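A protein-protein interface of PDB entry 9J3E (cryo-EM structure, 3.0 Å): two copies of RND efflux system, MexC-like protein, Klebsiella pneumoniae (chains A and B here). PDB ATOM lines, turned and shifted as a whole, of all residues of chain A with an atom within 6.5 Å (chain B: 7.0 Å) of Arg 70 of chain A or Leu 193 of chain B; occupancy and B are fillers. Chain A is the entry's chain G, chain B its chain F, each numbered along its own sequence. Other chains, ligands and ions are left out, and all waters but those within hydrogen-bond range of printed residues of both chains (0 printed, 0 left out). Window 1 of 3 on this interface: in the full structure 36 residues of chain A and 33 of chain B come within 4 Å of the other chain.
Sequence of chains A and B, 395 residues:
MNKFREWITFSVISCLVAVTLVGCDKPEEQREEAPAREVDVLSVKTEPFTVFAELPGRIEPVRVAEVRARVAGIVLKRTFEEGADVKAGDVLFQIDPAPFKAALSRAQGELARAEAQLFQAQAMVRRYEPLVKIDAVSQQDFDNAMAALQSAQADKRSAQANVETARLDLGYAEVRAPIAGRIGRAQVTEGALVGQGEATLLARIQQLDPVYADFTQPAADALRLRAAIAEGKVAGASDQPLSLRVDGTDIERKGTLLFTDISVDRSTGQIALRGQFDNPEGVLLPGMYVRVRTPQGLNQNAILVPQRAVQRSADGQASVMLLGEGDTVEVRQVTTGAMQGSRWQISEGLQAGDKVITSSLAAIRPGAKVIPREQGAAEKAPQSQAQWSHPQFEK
N of Val 64 of chain A sits at hydrogen-bond distance from OG1 of Thr 189 of chain B, at 2.9 Å.
The backbone NH (N) of Gly 191 of chain B lies within hydrogen-bond range of the backbone carbonyl oxygen (O) of Val 75 of chain B (2.7 Å).
The guanidinium group of Arg 68 of chain A lies within salt-bridge range of the side-chain carboxylate of Glu 66 of chain A (2.7 Å).
The guanidinium group of Arg 68 of chain A sits at hydrogen-bond distance from the backbone carbonyl oxygen of Ala 199 of chain A (3.0 Å).
NH2 of Arg 70 of chain A lies close to OH of Tyr 172 of chain A.
CB of Arg 68 of chain A touches CD2 of Leu 193 of chain B, 3.7 Å away.
NE of Arg 70 of chain A touches CD1 of Leu 193 of chain B (3.5 Å).
O of Arg 70 of chain A touches NE2 of Gln 196 of chain B (3.5 Å).
CD1 of Leu 168 of chain A touches CG of Pro 99 of chain B, 3.6 Å away.
Tyr 172 of chain A touches Pro 99 of chain B.
Pro 178 of chain A touches Gly 191 of chain B (CG to O, 3.4 Å).
Ala 199 of chain A touches Gln 196 of chain B.
Of chain A, only Arg 68 and Arg 70 come within 4 Å of Leu 193 of chain B.
Of the printed residues of chain B, Leu 168 of chain A touches Pro 99 (3.6 Å).
Of the printed residues of chain A, Gln 196 of chain B touches Arg 70 (3.5 Å) and Ala 199 (3.4 Å).
Printed residues of chain B within 4 Å of Tyr 172 of chain A: Pro 99.
Of the printed residues of chain B, Pro 178 of chain A touches Gly 191 (3.4 Å).
Of the printed residues of chain B, Arg 68 of chain A touches Leu 193 (3.7 Å).
Val 188 of chain B touches none of the printed residues of chain A.
The nearest residue of chain A that does not touch Leu 193 of chain B is Ala 199 of chain A (4.4 Å).
Among the printed residues, 8 pairs touch across the chains.
Among the printed residues, no Asp or Glu carboxylate lies within 4 Å of a Lys or Arg side-chain nitrogen of the other chain.
3 positions are printed for both chains.
Of the 8 pairs that touch across the chains among the printed residues, none has its exchanged pair printed and touching as well.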
ATOM      1  N   VAL A  64     -26.599 -19.719 -23.498  1.00  0.00           N
ATOM      2  CA  VAL A  64     -27.659 -18.897 -24.058  1.00  0.00           C
ATOM      3  C   VAL A  64     -27.311 -17.447 -23.780  1.00  0.00           C
ATOM      4  O   VAL A  64     -27.033 -17.081 -22.634  1.00  0.00           O
ATOM      5  CB  VAL A  64     -29.029 -19.241 -23.455  1.00  0.00           C
ATOM      6  CG1 VAL A  64     -30.141 -18.662 -24.309  1.00  0.00           C
ATOM      7  CG2 VAL A  64     -29.172 -20.732 -23.294  1.00  0.00           C
ATOM      8  N   ALA A  65     -27.328 -16.627 -24.819  1.00  0.00           N
ATOM      9  CA  ALA A  65     -27.023 -15.209 -24.697  1.00  0.00           C
ATOM     10  C   ALA A  65     -28.273 -14.419 -25.045  1.00  0.00           C
ATOM     11  O   ALA A  65     -28.521 -14.127 -26.218  1.00  0.00           O
ATOM     12  CB  ALA A  65     -25.860 -14.820 -25.604  1.00  0.00           C
ATOM     13  N   GLU A  66     -29.061 -14.075 -24.036  1.00  0.00           N
ATOM     14  CA  GLU A  66     -30.207 -13.197 -24.238  1.00  0.00           C
ATOM     15  C   GLU A  66     -29.657 -11.787 -24.366  1.00  0.00           C
ATOM     16  O   GLU A  66     -29.461 -11.082 -23.379  1.00  0.00           O
ATOM     17  CB  GLU A  66     -31.196 -13.321 -23.089  1.00  0.00           C
ATOM     18  CG  GLU A  66     -31.989 -14.607 -23.098  1.00  0.00           C
ATOM     19  CD  GLU A  66     -33.309 -14.472 -22.374  1.00  0.00           C
ATOM     20  OE1 GLU A  66     -33.494 -13.467 -21.658  1.00  0.00           O
ATOM     21  OE2 GLU A  66     -34.163 -15.372 -22.519  1.00  0.00           O
ATOM     22  N   VAL A  67     -29.383 -11.379 -25.601  1.00  0.00           N
ATOM     23  CA  VAL A  67     -28.808 -10.063 -25.858  1.00  0.00           C
ATOM     24  C   VAL A  67     -29.835  -9.011 -25.465  1.00  0.00           C
ATOM     25  O   VAL A  67     -30.934  -8.965 -26.023  1.00  0.00           O
ATOM     26  CB  VAL A  67     -28.392  -9.907 -27.320  1.00  0.00           C
ATOM     27  CG1 VAL A  67     -27.841  -8.537 -27.545  1.00  0.00           C
ATOM     28  CG2 VAL A  67     -27.367 -10.941 -27.681  1.00  0.00           C
ATOM     29  N   ARG A  68     -29.485  -8.159 -24.511  1.00  0.00           N
ATOM     30  CA  ARG A  68     -30.402  -7.154 -24.011  1.00  0.00           C
ATOM     31  C   ARG A  68     -29.811  -5.765 -24.179  1.00  0.00           C
ATOM     32  O   ARG A  68     -28.595  -5.590 -24.280  1.00  0.00           O
ATOM     33  CB  ARG A  68     -30.743  -7.403 -22.544  1.00  0.00           C
ATOM     34  CG  ARG A  68     -31.388  -8.742 -22.326  1.00  0.00           C
ATOM     35  CD  ARG A  68     -31.916  -8.898 -20.927  1.00  0.00           C
ATOM     36  NE  ARG A  68     -32.732 -10.099 -20.838  1.00  0.00           N
ATOM     37  CZ  ARG A  68     -34.055 -10.095 -20.821  1.00  0.00           C
ATOM     38  NH1 ARG A  68     -34.743  -8.969 -20.906  1.00  0.00           N
ATOM     39  NH2 ARG A  68     -34.706 -11.251 -20.737  1.00  0.00           N
ATOM     40  N   ALA A  69     -30.694  -4.776 -24.220  1.00  0.00           N
ATOM     41  CA  ALA A  69     -30.272  -3.390 -24.320  1.00  0.00           C
ATOM     42  C   ALA A  69     -29.868  -2.873 -22.949  1.00  0.00           C
ATOM     43  O   ALA A  69     -30.683  -2.840 -22.024  1.00  0.00           O
ATOM     44  CB  ALA A  69     -31.393  -2.532 -24.895  1.00  0.00           C
ATOM     45  N   ARG A  70     -28.607  -2.475 -22.816  1.00  0.00           N
ATOM     46  CA  ARG A  70     -28.127  -1.905 -21.569  1.00  0.00           C
ATOM     47  C   ARG A  70     -28.440  -0.426 -21.444  1.00  0.00           C
ATOM     48  O   ARG A  70     -28.287   0.138 -20.358  1.00  0.00           O
ATOM     49  CB  ARG A  70     -26.618  -2.105 -21.448  1.00  0.00           C
ATOM     50  CG  ARG A  70     -26.119  -3.351 -22.132  1.00  0.00           C
ATOM     51  CD  ARG A  70     -25.897  -4.462 -21.138  1.00  0.00           C
ATOM     52  NE  ARG A  70     -25.283  -3.976 -19.911  1.00  0.00           N
ATOM     53  CZ  ARG A  70     -23.976  -3.941 -19.698  1.00  0.00           C
ATOM     54  NH1 ARG A  70     -23.116  -4.351 -20.615  1.00  0.00           N
ATOM     55  NH2 ARG A  70     -23.520  -3.485 -18.536  1.00  0.00           N
ATOM     56  N   VAL A  71     -28.864   0.214 -22.529  1.00  0.00           N
ATOM     57  CA  VAL A  71     -29.082   1.649 -22.562  1.00  0.00           C
ATOM     58  C   VAL A  71     -30.406   1.934 -23.251  1.00  0.00           C
ATOM     59  O   VAL A  71     -30.935   1.113 -23.998  1.00  0.00           O
ATOM     60  CB  VAL A  71     -27.940   2.385 -23.284  1.00  0.00           C
ATOM     61  CG1 VAL A  71     -26.664   2.312 -22.473  1.00  0.00           C
ATOM     62  CG2 VAL A  71     -27.735   1.807 -24.666  1.00  0.00           C
ATOM     63  N   ALA A  72     -30.935   3.121 -22.991  1.00  0.00           N
ATOM     64  CA  ALA A  72     -32.181   3.551 -23.599  1.00  0.00           C
ATOM     65  C   ALA A  72     -31.904   4.269 -24.908  1.00  0.00           C
ATOM     66  O   ALA A  72     -31.012   5.115 -24.988  1.00  0.00           O
ATOM     67  CB  ALA A  72     -32.950   4.473 -22.656  1.00  0.00           C
ATOM     68  N   ILE A  95     -28.034   1.162 -31.457  1.00  0.00           N
ATOM     69  CA  ILE A  95     -28.885   2.072 -30.707  1.00  0.00           C
ATOM     70  C   ILE A  95     -28.372   3.486 -30.911  1.00  0.00           C
ATOM     71  O   ILE A  95     -27.159   3.719 -30.905  1.00  0.00           O
ATOM     72  CB  ILE A  95     -28.903   1.694 -29.217  1.00  0.00           C
ATOM     73  CG1 ILE A  95     -29.429   0.272 -29.048  1.00  0.00           C
ATOM     74  CG2 ILE A  95     -29.733   2.670 -28.433  1.00  0.00           C
ATOM     75  CD1 ILE A  95     -29.415  -0.205 -27.630  1.00  0.00           C
ATOM     76  N   LEU A 168     -17.147   3.189 -22.422  1.00  0.00           N
ATOM     77  CA  LEU A 168     -17.794   1.884 -22.340  1.00  0.00           C
ATOM     78  C   LEU A 168     -19.308   2.030 -22.306  1.00  0.00           C
ATOM     79  O   LEU A 168     -20.034   1.210 -22.886  1.00  0.00           O
ATOM     80  CB  LEU A 168     -17.271   1.113 -21.130  1.00  0.00           C
ATOM     81  CG  LEU A 168     -17.724   1.498 -19.728  1.00  0.00           C
ATOM     82  CD1 LEU A 168     -18.940   0.702 -19.309  1.00  0.00           C
ATOM     83  CD2 LEU A 168     -16.585   1.277 -18.756  1.00  0.00           C
ATOM     84  N   TYR A 172     -21.907   0.379 -25.047  1.00  0.00           N
ATOM     85  CA  TYR A 172     -23.142  -0.352 -24.782  1.00  0.00           C
ATOM     86  C   TYR A 172     -24.226  -0.059 -25.807  1.00  0.00           C
ATOM     87  O   TYR A 172     -25.128  -0.884 -25.977  1.00  0.00           O
ATOM     88  CB  TYR A 172     -23.673  -0.018 -23.392  1.00  0.00           C
ATOM     89  CG  TYR A 172     -22.865  -0.592 -22.263  1.00  0.00           C
ATOM     90  CD1 TYR A 172     -23.208  -0.338 -20.950  1.00  0.00           C
ATOM     91  CD2 TYR A 172     -21.764  -1.392 -22.508  1.00  0.00           C
ATOM     92  CE1 TYR A 172     -22.477  -0.852 -19.914  1.00  0.00           C
ATOM     93  CE2 TYR A 172     -21.025  -1.914 -21.476  1.00  0.00           C
ATOM     94  CZ  TYR A 172     -21.388  -1.642 -20.180  1.00  0.00           C
ATOM     95  OH  TYR A 172     -20.655  -2.163 -19.140  1.00  0.00           O
ATOM     96  N   ALA A 173     -24.166   1.086 -26.487  1.00  0.00           N
ATOM     97  CA  ALA A 173     -25.125   1.427 -27.527  1.00  0.00           C
ATOM     98  C   ALA A 173     -24.859   0.712 -28.841  1.00  0.00           C
ATOM     99  O   ALA A 173     -25.744   0.682 -29.701  1.00  0.00           O
ATOM    100  CB  ALA A 173     -25.132   2.938 -27.774  1.00  0.00           C
ATOM    101  N   PRO A 178     -22.332 -11.221 -27.349  1.00  0.00           N
ATOM    102  CA  PRO A 178     -21.389 -11.562 -26.281  1.00  0.00           C
ATOM    103  C   PRO A 178     -20.673 -12.876 -26.505  1.00  0.00           C
ATOM    104  O   PRO A 178     -19.496 -12.991 -26.148  1.00  0.00           O
ATOM    105  CB  PRO A 178     -22.279 -11.612 -25.037  1.00  0.00           C
ATOM    106  CG  PRO A 178     -23.615 -11.948 -25.565  1.00  0.00           C
ATOM    107  CD  PRO A 178     -23.728 -11.288 -26.897  1.00  0.00           C
ATOM    108  N   GLY A 195     -34.457  -0.353 -24.086  1.00  0.00           N
ATOM    109  CA  GLY A 195     -33.702   0.073 -22.935  1.00  0.00           C
ATOM    110  C   GLY A 195     -34.352   1.143 -22.091  1.00  0.00           C
ATOM    111  O   GLY A 195     -33.747   1.575 -21.104  1.00  0.00           O
ATOM    112  N   ALA A 199     -34.257  -3.546 -19.491  1.00  0.00           N
ATOM    113  CA  ALA A 199     -33.320  -4.058 -20.484  1.00  0.00           C
ATOM    114  C   ALA A 199     -34.101  -4.868 -21.504  1.00  0.00           C
ATOM    115  O   ALA A 199     -34.337  -6.062 -21.321  1.00  0.00           O
ATOM    116  CB  ALA A 199     -32.242  -4.900 -19.815  1.00  0.00           C
ATOM    117  N   THR A 200     -34.509  -4.212 -22.585  1.00  0.00           N
ATOM    118  CA  THR A 200     -35.350  -4.857 -23.580  1.00  0.00           C
ATOM    119  C   THR A 200     -34.609  -6.014 -24.232  1.00  0.00           C
ATOM    120  O   THR A 200     -33.464  -5.866 -24.666  1.00  0.00           O
ATOM    121  CB  THR A 200     -35.781  -3.848 -24.636  1.00  0.00           C
ATOM    122  OG1 THR A 200     -36.196  -2.637 -23.996  1.00  0.00           O
ATOM    123  CG2 THR A 200     -36.930  -4.396 -25.449  1.00  0.00           C
ATOM    124  N   LEU A 202     -33.378  -8.208 -27.002  1.00  0.00           N
ATOM    125  CA  LEU A 202     -33.178  -7.914 -28.411  1.00  0.00           C
ATOM    126  C   LEU A 202     -33.100  -9.175 -29.255  1.00  0.00           C
ATOM    127  O   LEU A 202     -33.753  -9.271 -30.296  1.00  0.00           O
ATOM    128  CB  LEU A 202     -31.918  -7.075 -28.590  1.00  0.00           C
ATOM    129  CG  LEU A 202     -31.861  -5.833 -27.711  1.00  0.00           C
ATOM    130  CD1 LEU A 202     -30.630  -5.026 -28.038  1.00  0.00           C
ATOM    131  CD2 LEU A 202     -33.105  -5.001 -27.917  1.00  0.00           C
ATOM    132  N   ALA B  72     -24.328  -5.145 -12.433  1.00  0.00           N
ATOM    133  CA  ALA B  72     -24.753  -5.400 -13.798  1.00  0.00           C
ATOM    134  C   ALA B  72     -23.554  -5.644 -14.702  1.00  0.00           C
ATOM    135  O   ALA B  72     -22.549  -4.934 -14.630  1.00  0.00           O
ATOM    136  CB  ALA B  72     -25.568  -4.223 -14.328  1.00  0.00           C
ATOM    137  N   GLY B  73     -23.665  -6.649 -15.557  1.00  0.00           N
ATOM    138  CA  GLY B  73     -22.605  -6.919 -16.504  1.00  0.00           C
ATOM    139  C   GLY B  73     -22.858  -8.209 -17.247  1.00  0.00           C
ATOM    140  O   GLY B  73     -23.893  -8.860 -17.089  1.00  0.00           O
ATOM    141  N   ILE B  74     -21.878  -8.565 -18.062  1.00  0.00           N
ATOM    142  CA  ILE B  74     -21.940  -9.758 -18.892  1.00  0.00           C
ATOM    143  C   ILE B  74     -21.137 -10.850 -18.208  1.00  0.00           C
ATOM    144  O   ILE B  74     -19.992 -10.626 -17.808  1.00  0.00           O
ATOM    145  CB  ILE B  74     -21.387  -9.469 -20.294  1.00  0.00           C
ATOM    146  CG1 ILE B  74     -22.432  -8.755 -21.147  1.00  0.00           C
ATOM    147  CG2 ILE B  74     -20.953 -10.750 -20.968  1.00  0.00           C
ATOM    148  CD1 ILE B  74     -23.717  -9.506 -21.297  1.00  0.00           C
ATOM    149  N   VAL B  75     -21.723 -12.037 -18.079  1.00  0.00           N
ATOM    150  CA  VAL B  75     -21.037 -13.124 -17.393  1.00  0.00           C
ATOM    151  C   VAL B  75     -19.899 -13.621 -18.268  1.00  0.00           C
ATOM    152  O   VAL B  75     -20.111 -14.404 -19.199  1.00  0.00           O
ATOM    153  CB  VAL B  75     -21.999 -14.269 -17.046  1.00  0.00           C
ATOM    154  CG1 VAL B  75     -21.259 -15.363 -16.314  1.00  0.00           C
ATOM    155  CG2 VAL B  75     -23.143 -13.752 -16.211  1.00  0.00           C
ATOM    156  N   ASP B  96     -17.800  -9.026 -16.169  1.00  0.00           N
ATOM    157  CA  ASP B  96     -16.782  -8.123 -16.698  1.00  0.00           C
ATOM    158  C   ASP B  96     -16.701  -6.857 -15.860  1.00  0.00           C
ATOM    159  O   ASP B  96     -17.716  -6.179 -15.670  1.00  0.00           O
ATOM    160  CB  ASP B  96     -17.046  -7.774 -18.161  1.00  0.00           C
ATOM    161  CG  ASP B  96     -18.395  -7.126 -18.383  1.00  0.00           C
ATOM    162  OD1 ASP B  96     -18.593  -6.533 -19.463  1.00  0.00           O
ATOM    163  OD2 ASP B  96     -19.268  -7.232 -17.500  1.00  0.00           O
ATOM    164  N   PRO B  99     -17.005  -1.170 -15.924  1.00  0.00           N
ATOM    165  CA  PRO B  99     -17.242   0.104 -15.238  1.00  0.00           C
ATOM    166  C   PRO B  99     -16.674   0.120 -13.830  1.00  0.00           C
ATOM    167  O   PRO B  99     -16.271   1.172 -13.327  1.00  0.00           O
ATOM    168  CB  PRO B  99     -18.773   0.218 -15.225  1.00  0.00           C
ATOM    169  CG  PRO B  99     -19.275  -0.922 -16.070  1.00  0.00           C
ATOM    170  CD  PRO B  99     -18.238  -1.968 -15.953  1.00  0.00           C
ATOM    171  N   PHE B 100     -16.634  -1.042 -13.182  1.00  0.00           N
ATOM    172  CA  PHE B 100     -16.176  -1.097 -11.800  1.00  0.00           C
ATOM    173  C   PHE B 100     -14.673  -0.895 -11.708  1.00  0.00           C
ATOM    174  O   PHE B 100     -14.182  -0.240 -10.782  1.00  0.00           O
ATOM    175  CB  PHE B 100     -16.592  -2.422 -11.180  1.00  0.00           C
ATOM    176  CG  PHE B 100     -17.909  -2.913 -11.679  1.00  0.00           C
ATOM    177  CD1 PHE B 100     -19.048  -2.151 -11.513  1.00  0.00           C
ATOM    178  CD2 PHE B 100     -18.007  -4.111 -12.354  1.00  0.00           C
ATOM    179  CE1 PHE B 100     -20.258  -2.585 -11.982  1.00  0.00           C
ATOM    180  CE2 PHE B 100     -19.215  -4.551 -12.827  1.00  0.00           C
ATOM    181  CZ  PHE B 100     -20.341  -3.785 -12.645  1.00  0.00           C
ATOM    182  N   VAL B 188     -27.438 -19.198 -14.981  1.00  0.00           N
ATOM    183  CA  VAL B 188     -27.073 -18.466 -16.184  1.00  0.00           C
ATOM    184  C   VAL B 188     -25.788 -19.057 -16.738  1.00  0.00           C
ATOM    185  O   VAL B 188     -25.007 -19.690 -16.027  1.00  0.00           O
ATOM    186  CB  VAL B 188     -26.897 -16.955 -15.933  1.00  0.00           C
ATOM    187  CG1 VAL B 188     -28.198 -16.340 -15.457  1.00  0.00           C
ATOM    188  CG2 VAL B 188     -25.795 -16.719 -14.924  1.00  0.00           C
ATOM    189  N   THR B 189     -25.579 -18.846 -18.028  1.00  0.00           N
ATOM    190  CA  THR B 189     -24.382 -19.297 -18.713  1.00  0.00           C
ATOM    191  C   THR B 189     -23.548 -18.097 -19.128  1.00  0.00           C
ATOM    192  O   THR B 189     -23.987 -16.949 -19.045  1.00  0.00           O
ATOM    193  CB  THR B 189     -24.746 -20.141 -19.933  1.00  0.00           C
ATOM    194  OG1 THR B 189     -25.494 -19.340 -20.853  1.00  0.00           O
ATOM    195  CG2 THR B 189     -25.595 -21.314 -19.507  1.00  0.00           C
ATOM    196  N   GLU B 190     -22.329 -18.377 -19.578  1.00  0.00           N
ATOM    197  CA  GLU B 190     -21.438 -17.309 -20.000  1.00  0.00           C
ATOM    198  C   GLU B 190     -22.065 -16.513 -21.135  1.00  0.00           C
ATOM    199  O   GLU B 190     -22.643 -17.078 -22.066  1.00  0.00           O
ATOM    200  CB  GLU B 190     -20.093 -17.878 -20.442  1.00  0.00           C
ATOM    201  CG  GLU B 190     -19.383 -18.683 -19.378  1.00  0.00           C
ATOM    202  CD  GLU B 190     -18.059 -19.236 -19.859  1.00  0.00           C
ATOM    203  OE1 GLU B 190     -17.785 -19.148 -21.074  1.00  0.00           O
ATOM    204  OE2 GLU B 190     -17.289 -19.754 -19.022  1.00  0.00           O
ATOM    205  N   GLY B 191     -21.951 -15.193 -21.052  1.00  0.00           N
ATOM    206  CA  GLY B 191     -22.508 -14.304 -22.044  1.00  0.00           C
ATOM    207  C   GLY B 191     -23.854 -13.720 -21.687  1.00  0.00           C
ATOM    208  O   GLY B 191     -24.300 -12.787 -22.361  1.00  0.00           O
ATOM    209  N   ALA B 192     -24.506 -14.222 -20.649  1.00  0.00           N
ATOM    210  CA  ALA B 192     -25.794 -13.686 -20.250  1.00  0.00           C
ATOM    211  C   ALA B 192     -25.619 -12.378 -19.492  1.00  0.00           C
ATOM    212  O   ALA B 192     -24.737 -12.241 -18.643  1.00  0.00           O
ATOM    213  CB  ALA B 192     -26.546 -14.690 -19.380  1.00  0.00           C
ATOM    214  N   LEU B 193     -26.477 -11.413 -19.803  1.00  0.00           N
ATOM    215  CA  LEU B 193     -26.474 -10.155 -19.073  1.00  0.00           C
ATOM    216  C   LEU B 193     -27.198 -10.336 -17.751  1.00  0.00           C
ATOM    217  O   LEU B 193     -28.376 -10.697 -17.725  1.00  0.00           O
ATOM    218  CB  LEU B 193     -27.146  -9.051 -19.883  1.00  0.00           C
ATOM    219  CG  LEU B 193     -27.449  -7.795 -19.069  1.00  0.00           C
ATOM    220  CD1 LEU B 193     -26.166  -7.112 -18.659  1.00  0.00           C
ATOM    221  CD2 LEU B 193     -28.339  -6.845 -19.835  1.00  0.00           C
ATOM    222  N   VAL B 194     -26.494 -10.077 -16.652  1.00  0.00           N
ATOM    223  CA  VAL B 194     -27.054 -10.232 -15.320  1.00  0.00           C
ATOM    224  C   VAL B 194     -26.846  -8.939 -14.553  1.00  0.00           C
ATOM    225  O   VAL B 194     -26.005  -8.111 -14.901  1.00  0.00           O
ATOM    226  CB  VAL B 194     -26.424 -11.406 -14.551  1.00  0.00           C
ATOM    227  CG1 VAL B 194     -26.570 -12.688 -15.332  1.00  0.00           C
ATOM    228  CG2 VAL B 194     -24.973 -11.117 -14.272  1.00  0.00           C
ATOM    229  N   GLY B 195     -27.635  -8.775 -13.498  1.00  0.00           N
ATOM    230  CA  GLY B 195     -27.483  -7.662 -12.590  1.00  0.00           C
ATOM    231  C   GLY B 195     -28.224  -6.401 -12.960  1.00  0.00           C
ATOM    232  O   GLY B 195     -28.225  -5.455 -12.165  1.00  0.00           O
ATOM    233  N   GLN B 196     -28.863  -6.347 -14.122  1.00  0.00           N
ATOM    234  CA  GLN B 196     -29.608  -5.164 -14.528  1.00  0.00           C
ATOM    235  C   GLN B 196     -31.045  -5.281 -14.048  1.00  0.00           C
ATOM    236  O   GLN B 196     -31.698  -6.303 -14.272  1.00  0.00           O
ATOM    237  CB  GLN B 196     -29.572  -4.976 -16.041  1.00  0.00           C
ATOM    238  CG  GLN B 196     -28.356  -4.236 -16.529  1.00  0.00           C
ATOM    239  CD  GLN B 196     -28.701  -3.196 -17.567  1.00  0.00           C
ATOM    240  OE1 GLN B 196     -29.789  -3.212 -18.138  1.00  0.00           O
ATOM    241  NE2 GLN B 196     -27.776  -2.279 -17.813  1.00  0.00           N
ATOM    242  N   GLU B 198     -32.796  -6.244 -11.584  1.00  0.00           N
ATOM    243  CA  GLU B 198     -32.941  -7.074 -10.402  1.00  0.00           C
ATOM    244  C   GLU B 198     -31.654  -7.837 -10.133  1.00  0.00           C
ATOM    245  O   GLU B 198     -30.804  -7.996 -11.012  1.00  0.00           O
ATOM    246  CB  GLU B 198     -34.099  -8.058 -10.575  1.00  0.00           C
ATOM    247  CG  GLU B 198     -33.682  -9.377 -11.197  1.00  0.00           C
ATOM    248  CD  GLU B 198     -33.407  -9.256 -12.684  1.00  0.00           C
ATOM    249  OE1 GLU B 198     -33.602  -8.158 -13.242  1.00  0.00           O
ATOM    250  OE2 GLU B 198     -32.992 -10.260 -13.299  1.00  0.00           O
ATOM    251  N   THR B 200     -30.019 -10.786 -10.345  1.00  0.00           N
ATOM    252  CA  THR B 200     -30.209 -12.037 -11.063  1.00  0.00           C
ATOM    253  C   THR B 200     -29.739 -13.209 -10.219  1.00  0.00           C
ATOM    254  O   THR B 200     -28.690 -13.143  -9.579  1.00  0.00           O
ATOM    255  CB  THR B 200     -29.440 -12.004 -12.381  1.00  0.00           C
ATOM    256  OG1 THR B 200     -29.713 -10.775 -13.064  1.00  0.00           O
ATOM    257  CG2 THR B 200     -29.843 -13.165 -13.260  1.00  0.00           C
